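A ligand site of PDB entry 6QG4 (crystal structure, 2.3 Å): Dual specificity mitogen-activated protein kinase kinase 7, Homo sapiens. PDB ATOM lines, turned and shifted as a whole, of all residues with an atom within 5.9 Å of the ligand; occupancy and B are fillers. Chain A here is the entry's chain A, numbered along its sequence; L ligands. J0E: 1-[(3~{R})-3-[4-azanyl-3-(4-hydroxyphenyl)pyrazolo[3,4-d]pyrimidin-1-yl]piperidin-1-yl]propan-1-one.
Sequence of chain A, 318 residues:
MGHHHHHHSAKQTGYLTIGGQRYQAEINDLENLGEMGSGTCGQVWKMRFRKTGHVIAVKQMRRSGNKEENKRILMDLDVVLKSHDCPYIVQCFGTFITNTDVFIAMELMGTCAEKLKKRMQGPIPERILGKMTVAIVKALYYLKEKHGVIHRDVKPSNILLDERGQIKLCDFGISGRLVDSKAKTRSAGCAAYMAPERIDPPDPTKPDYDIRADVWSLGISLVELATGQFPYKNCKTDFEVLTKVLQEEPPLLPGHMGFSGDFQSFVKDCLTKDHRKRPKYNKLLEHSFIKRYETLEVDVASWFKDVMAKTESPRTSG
Met 36 touches the ligand (O to C5, 3.2 Å).
O of Gly 37 touches C5 of the ligand (3.9 Å).
Ala 57 touches the ligand.
Lys 59 touches the ligand (CE to C14, 3.5 Å).
Val 90 touches the ligand.
Leu 108 touches the ligand.
Ser 157 touches the ligand.
Leu 160 touches the ligand.
Cys 170 touches the ligand.
Along chain A the residues within 4 Å of the ligand span positions 36 to 170.
The nearest printed residue that does not touch the ligand is Val 44 (4.1 Å).
The side-chain sulfur of Cys 112 is covalently linked to a carbon (C9) of the ligand (1.8 Å).
NZ of Lys 115 sits at hydrogen-bond distance from O of the ligand, 2.5 Å away.
An oxygen (O1) of the ligand is in hydrogen-bond range of the side-chain carboxylate (OD2) of Asp 76 (2.6 Å).
A nitrogen (N) of the ligand is in hydrogen-bond range of the backbone carbonyl oxygen (O) of Glu 107 (3.0 Å).
N of Met 109 sits at hydrogen-bond distance from N5 of the ligand.
The side-chain sulfur (SD) of Met 106 lies close to an oxygen (O1) of the ligand (3.5 Å).
SG of Cys 112 sits at hydrogen-bond distance from N of Lys 115.
O of Val 44 lies within hydrogen-bond range of N of Met 36 (2.9 Å).
The backbone NH (N) of Met 106 is in hydrogen-bond range of the backbone carbonyl oxygen (O) of Ala 57.
The backbone carbonyl oxygen (O) of Asn 158 is in hydrogen-bond range of the backbone NH (N) of Cys 170, 3.4 Å away.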
ATOM      1  N   MET A  36     -10.862  12.086  -4.854  1.00  0.00           N
ATOM      2  CA  MET A  36      -9.542  12.620  -5.141  1.00  0.00           C
ATOM      3  C   MET A  36      -8.844  11.698  -6.137  1.00  0.00           C
ATOM      4  O   MET A  36      -8.575  10.534  -5.829  1.00  0.00           O
ATOM      5  CB  MET A  36      -8.708  12.755  -3.867  1.00  0.00           C
ATOM      6  CG  MET A  36      -9.499  13.221  -2.657  1.00  0.00           C
ATOM      7  SD  MET A  36      -8.454  13.526  -1.215  1.00  0.00           S
ATOM      8  CE  MET A  36      -7.519  14.945  -1.781  1.00  0.00           C
ATOM      9  N   GLY A  37      -8.554  12.227  -7.322  1.00  0.00           N
ATOM     10  CA  GLY A  37      -7.868  11.468  -8.350  1.00  0.00           C
ATOM     11  C   GLY A  37      -8.654  10.259  -8.844  1.00  0.00           C
ATOM     12  O   GLY A  37      -8.267   9.116  -8.590  1.00  0.00           O
ATOM     13  N   VAL A  44     -10.510   7.059  -3.067  1.00  0.00           N
ATOM     14  CA  VAL A  44     -10.174   7.892  -1.915  1.00  0.00           C
ATOM     15  C   VAL A  44     -11.070   9.119  -1.945  1.00  0.00           C
ATOM     16  O   VAL A  44     -11.047   9.894  -2.906  1.00  0.00           O
ATOM     17  CB  VAL A  44      -8.693   8.291  -1.918  1.00  0.00           C
ATOM     18  CG1 VAL A  44      -8.378   9.160  -0.716  1.00  0.00           C
ATOM     19  CG2 VAL A  44      -7.810   7.041  -1.931  1.00  0.00           C
ATOM     20  N   ALA A  57      -9.045  12.455   4.533  1.00  0.00           N
ATOM     21  CA  ALA A  57      -9.081  11.567   3.386  1.00  0.00           C
ATOM     22  C   ALA A  57      -9.591  10.205   3.837  1.00  0.00           C
ATOM     23  O   ALA A  57      -9.154   9.689   4.871  1.00  0.00           O
ATOM     24  CB  ALA A  57      -7.694  11.436   2.745  1.00  0.00           C
ATOM     25  N   LYS A  59     -10.507   6.283   2.400  1.00  0.00           N
ATOM     26  CA  LYS A  59     -10.513   5.237   1.389  1.00  0.00           C
ATOM     27  C   LYS A  59     -11.639   4.264   1.675  1.00  0.00           C
ATOM     28  O   LYS A  59     -11.841   3.846   2.826  1.00  0.00           O
ATOM     29  CB  LYS A  59      -9.181   4.493   1.341  1.00  0.00           C
ATOM     30  CG  LYS A  59      -9.196   3.259   0.448  1.00  0.00           C
ATOM     31  CD  LYS A  59      -7.869   2.526   0.460  1.00  0.00           C
ATOM     32  CE  LYS A  59      -6.721   3.439   0.083  1.00  0.00           C
ATOM     33  NZ  LYS A  59      -5.592   2.692  -0.526  1.00  0.00           N
ATOM     34  N   ASP A  76      -1.792  -2.655   3.109  1.00  0.00           N
ATOM     35  CA  ASP A  76      -1.352  -1.273   3.286  1.00  0.00           C
ATOM     36  C   ASP A  76      -1.796  -0.737   4.645  1.00  0.00           C
ATOM     37  O   ASP A  76      -1.011  -0.112   5.366  1.00  0.00           O
ATOM     38  CB  ASP A  76      -1.891  -0.403   2.149  1.00  0.00           C
ATOM     39  CG  ASP A  76      -1.675   1.079   2.405  1.00  0.00           C
ATOM     40  OD1 ASP A  76      -0.504   1.526   2.336  1.00  0.00           O
ATOM     41  OD2 ASP A  76      -2.660   1.795   2.657  1.00  0.00           O
ATOM     42  N   LEU A  77      -3.059  -0.969   5.008  1.00  0.00           N
ATOM     43  CA  LEU A  77      -3.550  -0.505   6.296  1.00  0.00           C
ATOM     44  C   LEU A  77      -2.831  -1.197   7.446  1.00  0.00           C
ATOM     45  O   LEU A  77      -2.629  -0.587   8.507  1.00  0.00           O
ATOM     46  CB  LEU A  77      -5.057  -0.736   6.396  1.00  0.00           C
ATOM     47  CG  LEU A  77      -5.710  -0.461   7.754  1.00  0.00           C
ATOM     48  CD1 LEU A  77      -5.742   1.028   8.049  1.00  0.00           C
ATOM     49  CD2 LEU A  77      -7.117  -1.041   7.795  1.00  0.00           C
ATOM     50  N   VAL A  80       0.337   0.680   7.944  1.00  0.00           N
ATOM     51  CA  VAL A  80       0.039   2.033   8.401  1.00  0.00           C
ATOM     52  C   VAL A  80      -0.313   2.035   9.891  1.00  0.00           C
ATOM     53  O   VAL A  80       0.146   2.895  10.646  1.00  0.00           O
ATOM     54  CB  VAL A  80      -1.088   2.649   7.559  1.00  0.00           C
ATOM     55  CG1 VAL A  80      -1.627   3.909   8.222  1.00  0.00           C
ATOM     56  CG2 VAL A  80      -0.584   2.968   6.157  1.00  0.00           C
ATOM     57  N   VAL A  90       2.017   8.270   6.302  1.00  0.00           N
ATOM     58  CA  VAL A  90       0.653   8.797   6.434  1.00  0.00           C
ATOM     59  C   VAL A  90      -0.019   8.141   7.623  1.00  0.00           C
ATOM     60  O   VAL A  90      -0.132   6.903   7.698  1.00  0.00           O
ATOM     61  CB  VAL A  90      -0.128   8.576   5.142  1.00  0.00           C
ATOM     62  CG1 VAL A  90      -1.469   9.290   5.217  1.00  0.00           C
ATOM     63  CG2 VAL A  90       0.668   9.062   3.948  1.00  0.00           C
ATOM     64  N   MET A 106      -7.872   8.755   6.976  1.00  0.00           N
ATOM     65  CA  MET A 106      -6.442   9.019   6.969  1.00  0.00           C
ATOM     66  C   MET A 106      -6.179  10.515   6.969  1.00  0.00           C
ATOM     67  O   MET A 106      -7.078  11.327   6.733  1.00  0.00           O
ATOM     68  CB  MET A 106      -5.762   8.362   5.764  1.00  0.00           C
ATOM     69  CG  MET A 106      -5.872   6.852   5.732  1.00  0.00           C
ATOM     70  SD  MET A 106      -5.444   6.173   4.120  1.00  0.00           S
ATOM     71  CE  MET A 106      -6.563   7.084   3.064  1.00  0.00           C
ATOM     72  N   GLU A 107      -4.933  10.865   7.238  1.00  0.00           N
ATOM     73  CA  GLU A 107      -4.493  12.252   7.173  1.00  0.00           C
ATOM     74  C   GLU A 107      -4.603  12.769   5.746  1.00  0.00           C
ATOM     75  O   GLU A 107      -4.164  12.107   4.803  1.00  0.00           O
ATOM     76  CB  GLU A 107      -3.049  12.358   7.683  1.00  0.00           C
ATOM     77  CG  GLU A 107      -2.431  13.736   7.560  1.00  0.00           C
ATOM     78  CD  GLU A 107      -0.965  13.732   7.976  1.00  0.00           C
ATOM     79  OE1 GLU A 107      -0.402  12.626   8.133  1.00  0.00           O
ATOM     80  OE2 GLU A 107      -0.386  14.819   8.153  1.00  0.00           O
ATOM     81  N   LEU A 108      -5.189  13.957   5.591  1.00  0.00           N
ATOM     82  CA  LEU A 108      -5.395  14.531   4.266  1.00  0.00           C
ATOM     83  C   LEU A 108      -4.123  15.236   3.821  1.00  0.00           C
ATOM     84  O   LEU A 108      -3.752  16.283   4.364  1.00  0.00           O
ATOM     85  CB  LEU A 108      -6.585  15.499   4.285  1.00  0.00           C
ATOM     86  CG  LEU A 108      -6.871  16.201   2.958  1.00  0.00           C
ATOM     87  CD1 LEU A 108      -7.465  15.224   1.957  1.00  0.00           C
ATOM     88  CD2 LEU A 108      -7.802  17.386   3.163  1.00  0.00           C
ATOM     89  N   MET A 109      -3.450  14.678   2.823  1.00  0.00           N
ATOM     90  CA  MET A 109      -2.272  15.285   2.240  1.00  0.00           C
ATOM     91  C   MET A 109      -2.668  16.146   1.039  1.00  0.00           C
ATOM     92  O   MET A 109      -3.820  16.166   0.613  1.00  0.00           O
ATOM     93  CB  MET A 109      -1.260  14.226   1.830  1.00  0.00           C
ATOM     94  CG  MET A 109      -0.799  13.324   2.975  1.00  0.00           C
ATOM     95  SD  MET A 109       0.170  14.208   4.219  1.00  0.00           S
ATOM     96  CE  MET A 109       1.644  14.611   3.277  1.00  0.00           C
ATOM     97  N   GLY A 110      -1.686  16.860   0.498  1.00  0.00           N
ATOM     98  CA  GLY A 110      -1.932  17.707  -0.654  1.00  0.00           C
ATOM     99  C   GLY A 110      -1.983  16.927  -1.948  1.00  0.00           C
ATOM    100  O   GLY A 110      -3.071  16.657  -2.474  1.00  0.00           O
ATOM    101  N   THR A 111      -0.816  16.555  -2.470  1.00  0.00           N
ATOM    102  CA  THR A 111      -0.736  15.785  -3.707  1.00  0.00           C
ATOM    103  C   THR A 111       0.599  15.045  -3.704  1.00  0.00           C
ATOM    104  O   THR A 111       1.424  15.211  -2.803  1.00  0.00           O
ATOM    105  CB  THR A 111      -0.877  16.680  -4.944  1.00  0.00           C
ATOM    106  OG1 THR A 111      -1.022  15.861  -6.110  1.00  0.00           O
ATOM    107  CG2 THR A 111       0.350  17.570  -5.100  1.00  0.00           C
ATOM    108  N   CYS A 112       0.797  14.218  -4.727  1.00  0.00           N
ATOM    109  CA  CYS A 112       2.023  13.433  -4.852  1.00  0.00           C
ATOM    110  C   CYS A 112       3.078  14.205  -5.633  1.00  0.00           C
ATOM    111  O   CYS A 112       2.786  15.168  -6.340  1.00  0.00           O
ATOM    112  CB  CYS A 112       1.740  12.087  -5.522  1.00  0.00           C
ATOM    113  SG  CYS A 112       1.066  12.216  -7.184  1.00  0.00           S
ATOM    114  N   ALA A 113       4.337  13.759  -5.491  1.00  0.00           N
ATOM    115  CA  ALA A 113       5.435  14.417  -6.182  1.00  0.00           C
ATOM    116  C   ALA A 113       5.320  14.275  -7.699  1.00  0.00           C
ATOM    117  O   ALA A 113       5.827  15.122  -8.434  1.00  0.00           O
ATOM    118  CB  ALA A 113       6.772  13.854  -5.704  1.00  0.00           C
ATOM    119  N   GLU A 114       4.644  13.219  -8.170  1.00  0.00           N
ATOM    120  CA  GLU A 114       4.423  13.064  -9.600  1.00  0.00           C
ATOM    121  C   GLU A 114       3.546  14.178 -10.149  1.00  0.00           C
ATOM    122  O   GLU A 114       3.812  14.717 -11.235  1.00  0.00           O
ATOM    123  CB  GLU A 114       3.804  11.698  -9.889  1.00  0.00           C
ATOM    124  CG  GLU A 114       3.112  11.589 -11.235  1.00  0.00           C
ATOM    125  CD  GLU A 114       3.220  10.206 -11.838  1.00  0.00           C
ATOM    126  OE1 GLU A 114       4.338   9.826 -12.255  1.00  0.00           O
ATOM    127  OE2 GLU A 114       2.200   9.494 -11.897  1.00  0.00           O
ATOM    128  N   LYS A 115       2.498  14.556  -9.400  1.00  0.00           N
ATOM    129  CA  LYS A 115       1.655  15.662  -9.824  1.00  0.00           C
ATOM    130  C   LYS A 115       2.303  17.012  -9.562  1.00  0.00           C
ATOM    131  O   LYS A 115       1.982  17.992 -10.242  1.00  0.00           O
ATOM    132  CB  LYS A 115       0.298  15.583  -9.121  1.00  0.00           C
ATOM    133  CG  LYS A 115      -0.559  14.410  -9.571  1.00  0.00           C
ATOM    134  CD  LYS A 115      -1.954  14.860  -9.962  1.00  0.00           C
ATOM    135  CE  LYS A 115      -2.760  13.720 -10.554  1.00  0.00           C
ATOM    136  NZ  LYS A 115      -3.023  12.649  -9.560  1.00  0.00           N
ATOM    137  N   PRO A 156       7.771   8.600  -7.524  1.00  0.00           N
ATOM    138  CA  PRO A 156       7.217   9.925  -7.203  1.00  0.00           C
ATOM    139  C   PRO A 156       5.724   9.920  -6.896  1.00  0.00           C
ATOM    140  O   PRO A 156       5.268  10.762  -6.116  1.00  0.00           O
ATOM    141  CB  PRO A 156       7.534  10.742  -8.458  1.00  0.00           C
ATOM    142  CG  PRO A 156       8.741  10.102  -9.020  1.00  0.00           C
ATOM    143  CD  PRO A 156       8.577   8.636  -8.764  1.00  0.00           C
ATOM    144  N   SER A 157       4.955   9.003  -7.491  1.00  0.00           N
ATOM    145  CA  SER A 157       3.537   8.929  -7.189  1.00  0.00           C
ATOM    146  C   SER A 157       3.249   8.446  -5.769  1.00  0.00           C
ATOM    147  O   SER A 157       2.110   8.552  -5.311  1.00  0.00           O
ATOM    148  CB  SER A 157       2.833   8.020  -8.199  1.00  0.00           C
ATOM    149  OG  SER A 157       3.283   6.684  -8.080  1.00  0.00           O
ATOM    150  N   ASN A 158       4.257   7.910  -5.079  1.00  0.00           N
ATOM    151  CA  ASN A 158       4.099   7.433  -3.713  1.00  0.00           C
ATOM    152  C   ASN A 158       4.697   8.377  -2.674  1.00  0.00           C
ATOM    153  O   ASN A 158       4.846   7.990  -1.517  1.00  0.00           O
ATOM    154  CB  ASN A 158       4.732   6.045  -3.574  1.00  0.00           C
ATOM    155  CG  ASN A 158       3.871   4.949  -4.181  1.00  0.00           C
ATOM    156  OD1 ASN A 158       2.663   5.099  -4.314  1.00  0.00           O
ATOM    157  ND2 ASN A 158       4.500   3.838  -4.541  1.00  0.00           N
ATOM    158  N   ILE A 159       5.040   9.597  -3.074  1.00  0.00           N
ATOM    159  CA  ILE A 159       5.607  10.600  -2.176  1.00  0.00           C
ATOM    160  C   ILE A 159       4.597  11.725  -2.055  1.00  0.00           C
ATOM    161  O   ILE A 159       4.363  12.476  -3.009  1.00  0.00           O
ATOM    162  CB  ILE A 159       6.959  11.125  -2.692  1.00  0.00           C
ATOM    163  CG1 ILE A 159       7.926   9.965  -2.922  1.00  0.00           C
ATOM    164  CG2 ILE A 159       7.551  12.124  -1.701  1.00  0.00           C
ATOM    165  CD1 ILE A 159       9.188  10.357  -3.669  1.00  0.00           C
ATOM    166  N   LEU A 160       3.991  11.856  -0.871  1.00  0.00           N
ATOM    167  CA  LEU A 160       2.928  12.824  -0.645  1.00  0.00           C
ATOM    168  C   LEU A 160       3.462  14.079   0.031  1.00  0.00           C
ATOM    169  O   LEU A 160       4.286  13.999   0.958  1.00  0.00           O
ATOM    170  CB  LEU A 160       1.814  12.221   0.199  1.00  0.00           C
ATOM    171  CG  LEU A 160       1.079  11.020  -0.408  1.00  0.00           C
ATOM    172  CD1 LEU A 160      -0.123  10.638   0.448  1.00  0.00           C
ATOM    173  CD2 LEU A 160       0.658  11.313  -1.837  1.00  0.00           C
ATOM    174  N   CYS A 170       3.533   6.702   1.311  1.00  0.00           N
ATOM    175  CA  CYS A 170       2.121   6.332   1.445  1.00  0.00           C
ATOM    176  C   CYS A 170       1.852   4.860   1.163  1.00  0.00           C
ATOM    177  O   CYS A 170       1.419   4.146   2.066  1.00  0.00           O
ATOM    178  CB  CYS A 170       1.263   7.226   0.542  1.00  0.00           C
ATOM    179  SG  CYS A 170       1.388   6.879  -1.219  1.00  0.00           S
ATOM    180  N   ASP A 171       2.074   4.390  -0.059  1.00  0.00           N
ATOM    181  CA  ASP A 171       1.539   3.092  -0.475  1.00  0.00           C
ATOM    182  C   ASP A 171       2.435   1.953  -0.005  1.00  0.00           C
ATOM    183  O   ASP A 171       3.615   1.903  -0.355  1.00  0.00           O
ATOM    184  CB  ASP A 171       1.370   3.059  -1.992  1.00  0.00           C
ATOM    185  CG  ASP A 171       0.483   1.913  -2.454  1.00  0.00           C
ATOM    186  OD1 ASP A 171      -0.093   1.217  -1.588  1.00  0.00           O
ATOM    187  OD2 ASP A 171       0.367   1.705  -3.682  1.00  0.00           O
HETATM  188  N1  J0E L   1      -4.174  10.152  -2.270  1.00  0.00           N
HETATM  189  N2  J0E L   1      -3.209   9.799  -5.814  1.00  0.00           N
HETATM  190  C3  J0E L   1      -4.277  10.278  -3.750  1.00  0.00           C
HETATM  191  N4  J0E L   1      -4.544  12.348  -1.157  1.00  0.00           N
HETATM  192  C5  J0E L   1      -5.542   9.464  -5.764  1.00  0.00           C
HETATM  193  C6  J0E L   1      -4.244   8.926  -6.349  1.00  0.00           C
HETATM  194  C8  J0E L   1      -1.269  11.176  -6.014  1.00  0.00           C
HETATM  195  C11 J0E L   1      -3.825   8.844  -0.486  1.00  0.00           C
HETATM  196  C12 J0E L   1      -3.537   7.661   0.379  1.00  0.00           C
HETATM  197  C13 J0E L   1      -4.297   6.507   0.235  1.00  0.00           C
HETATM  198  C14 J0E L   1      -4.029   5.405   1.022  1.00  0.00           C
HETATM  199  C15 J0E L   1      -3.006   5.444   1.960  1.00  0.00           C
HETATM  200  C16 J0E L   1      -2.241   6.590   2.104  1.00  0.00           C
HETATM  201  C17 J0E L   1      -2.505   7.706   1.309  1.00  0.00           C
HETATM  202  C18 J0E L   1      -4.598  12.951   0.043  1.00  0.00           C
HETATM  203  N   J0E L   1      -3.952  10.336   2.433  1.00  0.00           N
HETATM  204  C   J0E L   1      -4.143  10.975   1.256  1.00  0.00           C
HETATM  205  O   J0E L   1      -2.833  10.896  -7.732  1.00  0.00           O
HETATM  206  C1  J0E L   1      -4.070  10.248  -0.040  1.00  0.00           C
HETATM  207  C10 J0E L   1      -3.007   9.718  -4.370  1.00  0.00           C
HETATM  208  C2  J0E L   1      -4.290  11.024  -1.264  1.00  0.00           C
HETATM  209  C4  J0E L   1      -5.485   9.479  -4.241  1.00  0.00           C
HETATM  210  C7  J0E L   1      -2.499  10.618  -6.595  1.00  0.00           C
HETATM  211  C9  J0E L   1       0.079  10.857  -6.651  1.00  0.00           C
HETATM  212  N3  J0E L   1      -3.900   8.847  -1.828  1.00  0.00           N
HETATM  213  N5  J0E L   1      -4.400  12.304   1.211  1.00  0.00           N
HETATM  214  O1  J0E L   1      -2.749   4.359   2.736  1.00  0.00           O
